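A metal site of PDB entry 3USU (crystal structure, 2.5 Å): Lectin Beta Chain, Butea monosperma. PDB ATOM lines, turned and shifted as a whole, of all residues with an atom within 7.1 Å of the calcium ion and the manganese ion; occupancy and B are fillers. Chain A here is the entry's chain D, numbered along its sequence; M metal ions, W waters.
A ring nitrogen (ND1) of His 143 is in hydrogen-bond range of the backbone carbonyl oxygen (O) of Asp 141, at 2.9 Å. The backbone carbonyl oxygen (O) of Gly 145 sits at hydrogen-bond distance from the backbone NH (N) of Glu 127.
Along chain A the residues within 4 Å of the calcium ion span positions 129 to 138. The nearest printed residue that does not touch the calcium ion is Asp 89 (4.04 Å).
Four residues have an atom within 4 Å of the manganese ion: Glu 127, Asp 129, Asp 138 and His 143.
Water W1 binds the calcium ion (2.1 Å). OD1 of Asn 133 binds the calcium ion, at 2.2 Å. O of Tyr 131 binds the calcium ion (2.3 Å). Water W3 binds the calcium ion. OD2 of Asp 129 binds the calcium ion, 2.5 Å away. OD1 of Asp 129 binds the calcium ion, at 2.5 Å. The side-chain carboxylate (OD1) of Asp 138 is bound to the calcium ion, at 2.8 Å.
The manganese ion is bound by a ring nitrogen (NE2) of His 143 (2.1 Å), the side-chain carboxylate (OD2) of Asp 138 (2.1 Å), water W2 (2.2 Å), the side-chain carboxylate (OE2) of Glu 127 (2.3 Å), water W4 (2.3 Å) and the side-chain carboxylate (OD1) of Asp 129 (2.3 Å).
Water W2 lies within hydrogen-bond range of the side-chain carboxylate of Glu 127 (2.6 Å) and the backbone carbonyl oxygen of Ile 151 (3.0 Å).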
ATOM      1  N   ASP A  89     -26.259 -31.289 -11.599  1.00  0.00           N
ATOM      2  CA  ASP A  89     -26.082 -29.954 -11.019  1.00  0.00           C
ATOM      3  C   ASP A  89     -27.330 -29.433 -10.312  1.00  0.00           C
ATOM      4  O   ASP A  89     -27.231 -28.710  -9.321  1.00  0.00           O
ATOM      5  CB  ASP A  89     -25.545 -28.949 -12.047  1.00  0.00           C
ATOM      6  CG  ASP A  89     -24.125 -28.576 -11.773  1.00  0.00           C
ATOM      7  OD1 ASP A  89     -23.866 -27.807 -10.814  1.00  0.00           O
ATOM      8  OD2 ASP A  89     -23.237 -29.069 -12.507  1.00  0.00           O
ATOM      9  N   GLY A  90     -28.490 -29.847 -10.839  1.00  0.00           N
ATOM     10  CA  GLY A  90     -29.783 -29.634 -10.201  1.00  0.00           C
ATOM     11  C   GLY A  90     -30.932 -29.335 -11.161  1.00  0.00           C
ATOM     12  O   GLY A  90     -30.768 -29.425 -12.366  1.00  0.00           O
ATOM     13  N   ALA A 106     -24.637 -27.334 -16.486  1.00  0.00           N
ATOM     14  CA  ALA A 106     -24.072 -27.442 -15.146  1.00  0.00           C
ATOM     15  C   ALA A 106     -24.640 -26.326 -14.247  1.00  0.00           C
ATOM     16  O   ALA A 106     -25.815 -25.994 -14.331  1.00  0.00           O
ATOM     17  CB  ALA A 106     -22.550 -27.334 -15.182  1.00  0.00           C
ATOM     18  N   GLY A 107     -23.778 -25.781 -13.378  1.00  0.00           N
ATOM     19  CA  GLY A 107     -24.161 -24.840 -12.318  1.00  0.00           C
ATOM     20  C   GLY A 107     -25.172 -23.819 -12.773  1.00  0.00           C
ATOM     21  O   GLY A 107     -26.027 -23.376 -11.999  1.00  0.00           O
ATOM     22  N   PHE A 108     -25.091 -23.453 -14.057  1.00  0.00           N
ATOM     23  CA  PHE A 108     -25.983 -22.472 -14.640  1.00  0.00           C
ATOM     24  C   PHE A 108     -27.436 -22.941 -14.669  1.00  0.00           C
ATOM     25  O   PHE A 108     -28.348 -22.098 -14.766  1.00  0.00           O
ATOM     26  CB  PHE A 108     -25.498 -22.078 -16.026  1.00  0.00           C
ATOM     27  CG  PHE A 108     -24.023 -21.745 -16.069  1.00  0.00           C
ATOM     28  CD1 PHE A 108     -23.546 -20.559 -15.536  1.00  0.00           C
ATOM     29  CD2 PHE A 108     -23.106 -22.646 -16.604  1.00  0.00           C
ATOM     30  CE1 PHE A 108     -22.194 -20.269 -15.554  1.00  0.00           C
ATOM     31  CE2 PHE A 108     -21.754 -22.360 -16.635  1.00  0.00           C
ATOM     32  CZ  PHE A 108     -21.305 -21.169 -16.104  1.00  0.00           C
ATOM     33  N   LEU A 109     -27.649 -24.257 -14.587  1.00  0.00           N
ATOM     34  CA  LEU A 109     -28.973 -24.910 -14.496  1.00  0.00           C
ATOM     35  C   LEU A 109     -29.789 -24.657 -15.766  1.00  0.00           C
ATOM     36  O   LEU A 109     -31.037 -24.776 -15.786  1.00  0.00           O
ATOM     37  CB  LEU A 109     -29.701 -24.499 -13.201  1.00  0.00           C
ATOM     38  CG  LEU A 109     -28.962 -24.851 -11.880  1.00  0.00           C
ATOM     39  CD1 LEU A 109     -29.780 -24.466 -10.637  1.00  0.00           C
ATOM     40  CD2 LEU A 109     -28.592 -26.336 -11.841  1.00  0.00           C
ATOM     41  N   GLU A 127     -34.410 -22.694  -7.422  1.00  0.00           N
ATOM     42  CA  GLU A 127     -33.498 -23.812  -7.677  1.00  0.00           C
ATOM     43  C   GLU A 127     -33.478 -24.909  -6.601  1.00  0.00           C
ATOM     44  O   GLU A 127     -33.725 -24.678  -5.391  1.00  0.00           O
ATOM     45  CB  GLU A 127     -32.079 -23.312  -7.952  1.00  0.00           C
ATOM     46  CG  GLU A 127     -31.575 -22.258  -7.007  1.00  0.00           C
ATOM     47  CD  GLU A 127     -30.090 -22.256  -6.947  1.00  0.00           C
ATOM     48  OE1 GLU A 127     -29.439 -21.813  -7.923  1.00  0.00           O
ATOM     49  OE2 GLU A 127     -29.576 -22.763  -5.945  1.00  0.00           O
ATOM     50  N   PHE A 128     -33.199 -26.119  -7.086  1.00  0.00           N
ATOM     51  CA  PHE A 128     -32.920 -27.270  -6.275  1.00  0.00           C
ATOM     52  C   PHE A 128     -31.529 -27.666  -6.720  1.00  0.00           C
ATOM     53  O   PHE A 128     -31.351 -28.371  -7.731  1.00  0.00           O
ATOM     54  CB  PHE A 128     -33.999 -28.345  -6.475  1.00  0.00           C
ATOM     55  CG  PHE A 128     -35.379 -27.830  -6.142  1.00  0.00           C
ATOM     56  CD1 PHE A 128     -35.917 -28.021  -4.867  1.00  0.00           C
ATOM     57  CD2 PHE A 128     -36.097 -27.072  -7.068  1.00  0.00           C
ATOM     58  CE1 PHE A 128     -37.154 -27.508  -4.520  1.00  0.00           C
ATOM     59  CE2 PHE A 128     -37.360 -26.548  -6.738  1.00  0.00           C
ATOM     60  CZ  PHE A 128     -37.874 -26.763  -5.458  1.00  0.00           C
ATOM     61  N   ASP A 129     -30.558 -27.137  -5.972  1.00  0.00           N
ATOM     62  CA  ASP A 129     -29.138 -27.142  -6.323  1.00  0.00           C
ATOM     63  C   ASP A 129     -28.393 -28.215  -5.523  1.00  0.00           C
ATOM     64  O   ASP A 129     -28.503 -28.303  -4.279  1.00  0.00           O
ATOM     65  CB  ASP A 129     -28.589 -25.757  -6.052  1.00  0.00           C
ATOM     66  CG  ASP A 129     -27.174 -25.575  -6.547  1.00  0.00           C
ATOM     67  OD1 ASP A 129     -26.847 -24.440  -6.930  1.00  0.00           O
ATOM     68  OD2 ASP A 129     -26.366 -26.533  -6.540  1.00  0.00           O
ATOM     69  N   THR A 130     -27.612 -29.027  -6.236  1.00  0.00           N
ATOM     70  CA  THR A 130     -27.046 -30.236  -5.688  1.00  0.00           C
ATOM     71  C   THR A 130     -25.532 -30.255  -5.739  1.00  0.00           C
ATOM     72  O   THR A 130     -24.893 -31.238  -5.328  1.00  0.00           O
ATOM     73  CB  THR A 130     -27.597 -31.475  -6.425  1.00  0.00           C
ATOM     74  OG1 THR A 130     -27.376 -31.320  -7.836  1.00  0.00           O
ATOM     75  CG2 THR A 130     -29.102 -31.680  -6.107  1.00  0.00           C
ATOM     76  N   TYR A 131     -24.938 -29.182  -6.225  1.00  0.00           N
ATOM     77  CA  TYR A 131     -23.516 -29.122  -6.330  1.00  0.00           C
ATOM     78  C   TYR A 131     -23.022 -27.744  -5.949  1.00  0.00           C
ATOM     79  O   TYR A 131     -23.602 -26.755  -6.377  1.00  0.00           O
ATOM     80  CB  TYR A 131     -23.116 -29.464  -7.770  1.00  0.00           C
ATOM     81  CG  TYR A 131     -21.647 -29.331  -8.021  1.00  0.00           C
ATOM     82  CD1 TYR A 131     -20.795 -30.440  -7.952  1.00  0.00           C
ATOM     83  CD2 TYR A 131     -21.101 -28.087  -8.342  1.00  0.00           C
ATOM     84  CE1 TYR A 131     -19.432 -30.297  -8.198  1.00  0.00           C
ATOM     85  CE2 TYR A 131     -19.745 -27.942  -8.582  1.00  0.00           C
ATOM     86  CZ  TYR A 131     -18.905 -29.039  -8.515  1.00  0.00           C
ATOM     87  OH  TYR A 131     -17.549 -28.855  -8.771  1.00  0.00           O
ATOM     88  N   GLU A 132     -21.958 -27.663  -5.174  1.00  0.00           N
ATOM     89  CA  GLU A 132     -21.528 -26.358  -4.755  1.00  0.00           C
ATOM     90  C   GLU A 132     -20.622 -25.607  -5.729  1.00  0.00           C
ATOM     91  O   GLU A 132     -19.506 -26.018  -6.003  1.00  0.00           O
ATOM     92  CB  GLU A 132     -20.931 -26.357  -3.367  1.00  0.00           C
ATOM     93  CG  GLU A 132     -20.477 -24.965  -3.003  1.00  0.00           C
ATOM     94  CD  GLU A 132     -19.688 -24.921  -1.734  1.00  0.00           C
ATOM     95  OE1 GLU A 132     -19.357 -26.000  -1.213  1.00  0.00           O
ATOM     96  OE2 GLU A 132     -19.407 -23.795  -1.260  1.00  0.00           O
ATOM     97  N   ASN A 133     -21.118 -24.485  -6.244  1.00  0.00           N
ATOM     98  CA  ASN A 133     -20.345 -23.612  -7.106  1.00  0.00           C
ATOM     99  C   ASN A 133     -19.954 -22.474  -6.208  1.00  0.00           C
ATOM    100  O   ASN A 133     -20.758 -21.649  -5.780  1.00  0.00           O
ATOM    101  CB  ASN A 133     -21.185 -23.117  -8.292  1.00  0.00           C
ATOM    102  CG  ASN A 133     -21.706 -24.259  -9.174  1.00  0.00           C
ATOM    103  OD1 ASN A 133     -22.867 -24.668  -9.073  1.00  0.00           O
ATOM    104  ND2 ASN A 133     -20.852 -24.765 -10.043  1.00  0.00           N
ATOM    105  N   THR A 134     -18.682 -22.486  -5.869  1.00  0.00           N
ATOM    106  CA  THR A 134     -18.068 -21.543  -4.958  1.00  0.00           C
ATOM    107  C   THR A 134     -17.892 -20.204  -5.719  1.00  0.00           C
ATOM    108  O   THR A 134     -18.044 -19.118  -5.170  1.00  0.00           O
ATOM    109  CB  THR A 134     -16.733 -22.155  -4.501  1.00  0.00           C
ATOM    110  OG1 THR A 134     -15.855 -21.144  -4.004  1.00  0.00           O
ATOM    111  CG2 THR A 134     -16.051 -22.886  -5.681  1.00  0.00           C
ATOM    112  N   PHE A 136     -20.091 -19.225  -7.529  1.00  0.00           N
ATOM    113  CA  PHE A 136     -21.431 -18.621  -7.463  1.00  0.00           C
ATOM    114  C   PHE A 136     -21.881 -18.196  -6.063  1.00  0.00           C
ATOM    115  O   PHE A 136     -22.982 -17.691  -5.918  1.00  0.00           O
ATOM    116  CB  PHE A 136     -22.510 -19.595  -8.004  1.00  0.00           C
ATOM    117  CG  PHE A 136     -22.297 -20.022  -9.424  1.00  0.00           C
ATOM    118  CD1 PHE A 136     -21.396 -19.357 -10.277  1.00  0.00           C
ATOM    119  CD2 PHE A 136     -23.007 -21.100  -9.943  1.00  0.00           C
ATOM    120  CE1 PHE A 136     -21.204 -19.758 -11.593  1.00  0.00           C
ATOM    121  CE2 PHE A 136     -22.815 -21.501 -11.260  1.00  0.00           C
ATOM    122  CZ  PHE A 136     -21.906 -20.829 -12.078  1.00  0.00           C
ATOM    123  N   LEU A 137     -21.059 -18.421  -5.039  1.00  0.00           N
ATOM    124  CA  LEU A 137     -21.446 -18.253  -3.619  1.00  0.00           C
ATOM    125  C   LEU A 137     -22.462 -19.279  -3.127  1.00  0.00           C
ATOM    126  O   LEU A 137     -23.195 -19.008  -2.185  1.00  0.00           O
ATOM    127  CB  LEU A 137     -21.923 -16.817  -3.313  1.00  0.00           C
ATOM    128  CG  LEU A 137     -20.934 -15.642  -3.294  1.00  0.00           C
ATOM    129  CD1 LEU A 137     -19.550 -15.998  -2.771  1.00  0.00           C
ATOM    130  CD2 LEU A 137     -20.868 -15.013  -4.672  1.00  0.00           C
ATOM    131  N   ASP A 138     -22.518 -20.458  -3.749  1.00  0.00           N
ATOM    132  CA  ASP A 138     -23.418 -21.510  -3.231  1.00  0.00           C
ATOM    133  C   ASP A 138     -23.100 -21.862  -1.792  1.00  0.00           C
ATOM    134  O   ASP A 138     -21.956 -22.030  -1.462  1.00  0.00           O
ATOM    135  CB  ASP A 138     -23.305 -22.790  -4.026  1.00  0.00           C
ATOM    136  CG  ASP A 138     -24.056 -22.740  -5.310  1.00  0.00           C
ATOM    137  OD1 ASP A 138     -23.454 -23.156  -6.313  1.00  0.00           O
ATOM    138  OD2 ASP A 138     -25.228 -22.306  -5.358  1.00  0.00           O
ATOM    139  N   PRO A 139     -24.129 -22.027  -0.948  1.00  0.00           N
ATOM    140  CA  PRO A 139     -23.786 -22.640   0.324  1.00  0.00           C
ATOM    141  C   PRO A 139     -23.186 -24.025   0.064  1.00  0.00           C
ATOM    142  O   PRO A 139     -23.419 -24.621  -0.984  1.00  0.00           O
ATOM    143  CB  PRO A 139     -25.130 -22.741   1.053  1.00  0.00           C
ATOM    144  CG  PRO A 139     -26.163 -22.666  -0.024  1.00  0.00           C
ATOM    145  CD  PRO A 139     -25.568 -21.731  -1.038  1.00  0.00           C
ATOM    146  N   ASP A 141     -23.890 -26.695   1.426  1.00  0.00           N
ATOM    147  CA  ASP A 141     -24.981 -27.639   1.567  1.00  0.00           C
ATOM    148  C   ASP A 141     -25.755 -27.692   0.270  1.00  0.00           C
ATOM    149  O   ASP A 141     -25.861 -26.675  -0.440  1.00  0.00           O
ATOM    150  CB  ASP A 141     -25.897 -27.110   2.676  1.00  0.00           C
ATOM    151  CG  ASP A 141     -25.119 -26.458   3.818  1.00  0.00           C
ATOM    152  OD1 ASP A 141     -24.672 -27.246   4.716  1.00  0.00           O
ATOM    153  OD2 ASP A 141     -24.955 -25.192   3.841  1.00  0.00           O
ATOM    154  N   HIS A 143     -29.069 -27.353  -1.641  1.00  0.00           N
ATOM    155  CA  HIS A 143     -29.932 -26.251  -1.238  1.00  0.00           C
ATOM    156  C   HIS A 143     -31.119 -25.913  -2.149  1.00  0.00           C
ATOM    157  O   HIS A 143     -31.130 -26.221  -3.355  1.00  0.00           O
ATOM    158  CB  HIS A 143     -29.066 -24.995  -1.005  1.00  0.00           C
ATOM    159  CG  HIS A 143     -28.270 -24.558  -2.220  1.00  0.00           C
ATOM    160  ND1 HIS A 143     -27.114 -25.115  -2.557  1.00  0.00           N
ATOM    161  CD2 HIS A 143     -28.517 -23.578  -3.168  1.00  0.00           C
ATOM    162  CE1 HIS A 143     -26.627 -24.537  -3.671  1.00  0.00           C
ATOM    163  NE2 HIS A 143     -27.500 -23.607  -4.048  1.00  0.00           N
ATOM    164  N   ILE A 144     -32.126 -25.274  -1.556  1.00  0.00           N
ATOM    165  CA  ILE A 144     -33.180 -24.589  -2.291  1.00  0.00           C
ATOM    166  C   ILE A 144     -32.791 -23.112  -2.301  1.00  0.00           C
ATOM    167  O   ILE A 144     -32.525 -22.530  -1.243  1.00  0.00           O
ATOM    168  CB  ILE A 144     -34.550 -24.811  -1.614  1.00  0.00           C
ATOM    169  CG1 ILE A 144     -35.011 -26.252  -1.829  1.00  0.00           C
ATOM    170  CG2 ILE A 144     -35.599 -23.855  -2.156  1.00  0.00           C
ATOM    171  CD1 ILE A 144     -36.051 -26.735  -0.835  1.00  0.00           C
ATOM    172  N   GLY A 145     -32.710 -22.528  -3.495  1.00  0.00           N
ATOM    173  CA  GLY A 145     -32.381 -21.088  -3.627  1.00  0.00           C
ATOM    174  C   GLY A 145     -33.386 -20.310  -4.470  1.00  0.00           C
ATOM    175  O   GLY A 145     -34.089 -20.885  -5.296  1.00  0.00           O
ATOM    176  N   ASP A 147     -33.493 -17.435  -7.258  1.00  0.00           N
ATOM    177  CA  ASP A 147     -32.640 -16.639  -8.125  1.00  0.00           C
ATOM    178  C   ASP A 147     -33.422 -15.550  -8.835  1.00  0.00           C
ATOM    179  O   ASP A 147     -34.567 -15.772  -9.231  1.00  0.00           O
ATOM    180  CB  ASP A 147     -31.931 -17.554  -9.127  1.00  0.00           C
ATOM    181  CG  ASP A 147     -31.293 -18.770  -8.454  1.00  0.00           C
ATOM    182  OD1 ASP A 147     -31.031 -18.712  -7.229  1.00  0.00           O
ATOM    183  OD2 ASP A 147     -31.075 -19.798  -9.154  1.00  0.00           O
ATOM    184  N   ILE A 151     -27.582 -16.580 -11.082  1.00  0.00           N
ATOM    185  CA  ILE A 151     -27.457 -17.876 -10.490  1.00  0.00           C
ATOM    186  C   ILE A 151     -26.885 -17.772  -9.081  1.00  0.00           C
ATOM    187  O   ILE A 151     -26.950 -18.681  -8.307  1.00  0.00           O
ATOM    188  CB  ILE A 151     -26.560 -18.719 -11.386  1.00  0.00           C
ATOM    189  CG1 ILE A 151     -26.448 -20.145 -10.874  1.00  0.00           C
ATOM    190  CG2 ILE A 151     -25.208 -18.077 -11.504  1.00  0.00           C
ATOM    191  CD1 ILE A 151     -27.699 -20.941 -10.947  1.00  0.00           C
ATOM    192  N   LYS A 152     -26.328 -16.618  -8.767  1.00  0.00           N
ATOM    193  CA  LYS A 152     -25.968 -16.297  -7.398  1.00  0.00           C
ATOM    194  C   LYS A 152     -27.232 -15.979  -6.638  1.00  0.00           C
ATOM    195  O   LYS A 152     -27.713 -14.829  -6.638  1.00  0.00           O
ATOM    196  CB  LYS A 152     -24.993 -15.141  -7.295  1.00  0.00           C
ATOM    197  CG  LYS A 152     -24.864 -14.607  -5.864  1.00  0.00           C
ATOM    198  CD  LYS A 152     -23.776 -13.541  -5.742  1.00  0.00           C
ATOM    199  CE  LYS A 152     -23.902 -12.732  -4.451  1.00  0.00           C
ATOM    200  NZ  LYS A 152     -23.581 -13.516  -3.220  1.00  0.00           N
ATOM    201  N   SER A 153     -27.773 -17.010  -6.010  1.00  0.00           N
ATOM    202  CA  SER A 153     -29.028 -16.938  -5.319  1.00  0.00           C
ATOM    203  C   SER A 153     -29.144 -15.828  -4.261  1.00  0.00           C
ATOM    204  O   SER A 153     -28.244 -15.658  -3.454  1.00  0.00           O
ATOM    205  CB  SER A 153     -29.281 -18.293  -4.692  1.00  0.00           C
ATOM    206  OG  SER A 153     -30.450 -18.255  -3.943  1.00  0.00           O
ATOM    207  N   THR A 156     -30.903 -18.717   0.253  1.00  0.00           N
ATOM    208  CA  THR A 156     -30.902 -20.169   0.133  1.00  0.00           C
ATOM    209  C   THR A 156     -31.259 -20.823   1.489  1.00  0.00           C
ATOM    210  O   THR A 156     -30.948 -20.270   2.546  1.00  0.00           O
ATOM    211  CB  THR A 156     -29.528 -20.711  -0.374  1.00  0.00           C
ATOM    212  OG1 THR A 156     -28.540 -20.601   0.656  1.00  0.00           O
ATOM    213  CG2 THR A 156     -29.025 -19.966  -1.569  1.00  0.00           C
HETATM  214 CA    CA M   1     -24.604 -25.257  -7.770  1.00  0.00          CA
HETATM  215 MN    MN M   2     -27.316 -22.463  -5.773  1.00  0.00          MN
HETATM  216  O   HOH W   1     -25.213 -26.718  -9.182  1.00  0.00           O
HETATM  217  O   HOH W   2     -26.839 -21.659  -7.756  1.00  0.00           O
HETATM  218  O   HOH W   3     -25.419 -23.738  -9.473  1.00  0.00           O
HETATM  219  O   HOH W   4     -27.325 -20.628  -4.362  1.00  0.00           O
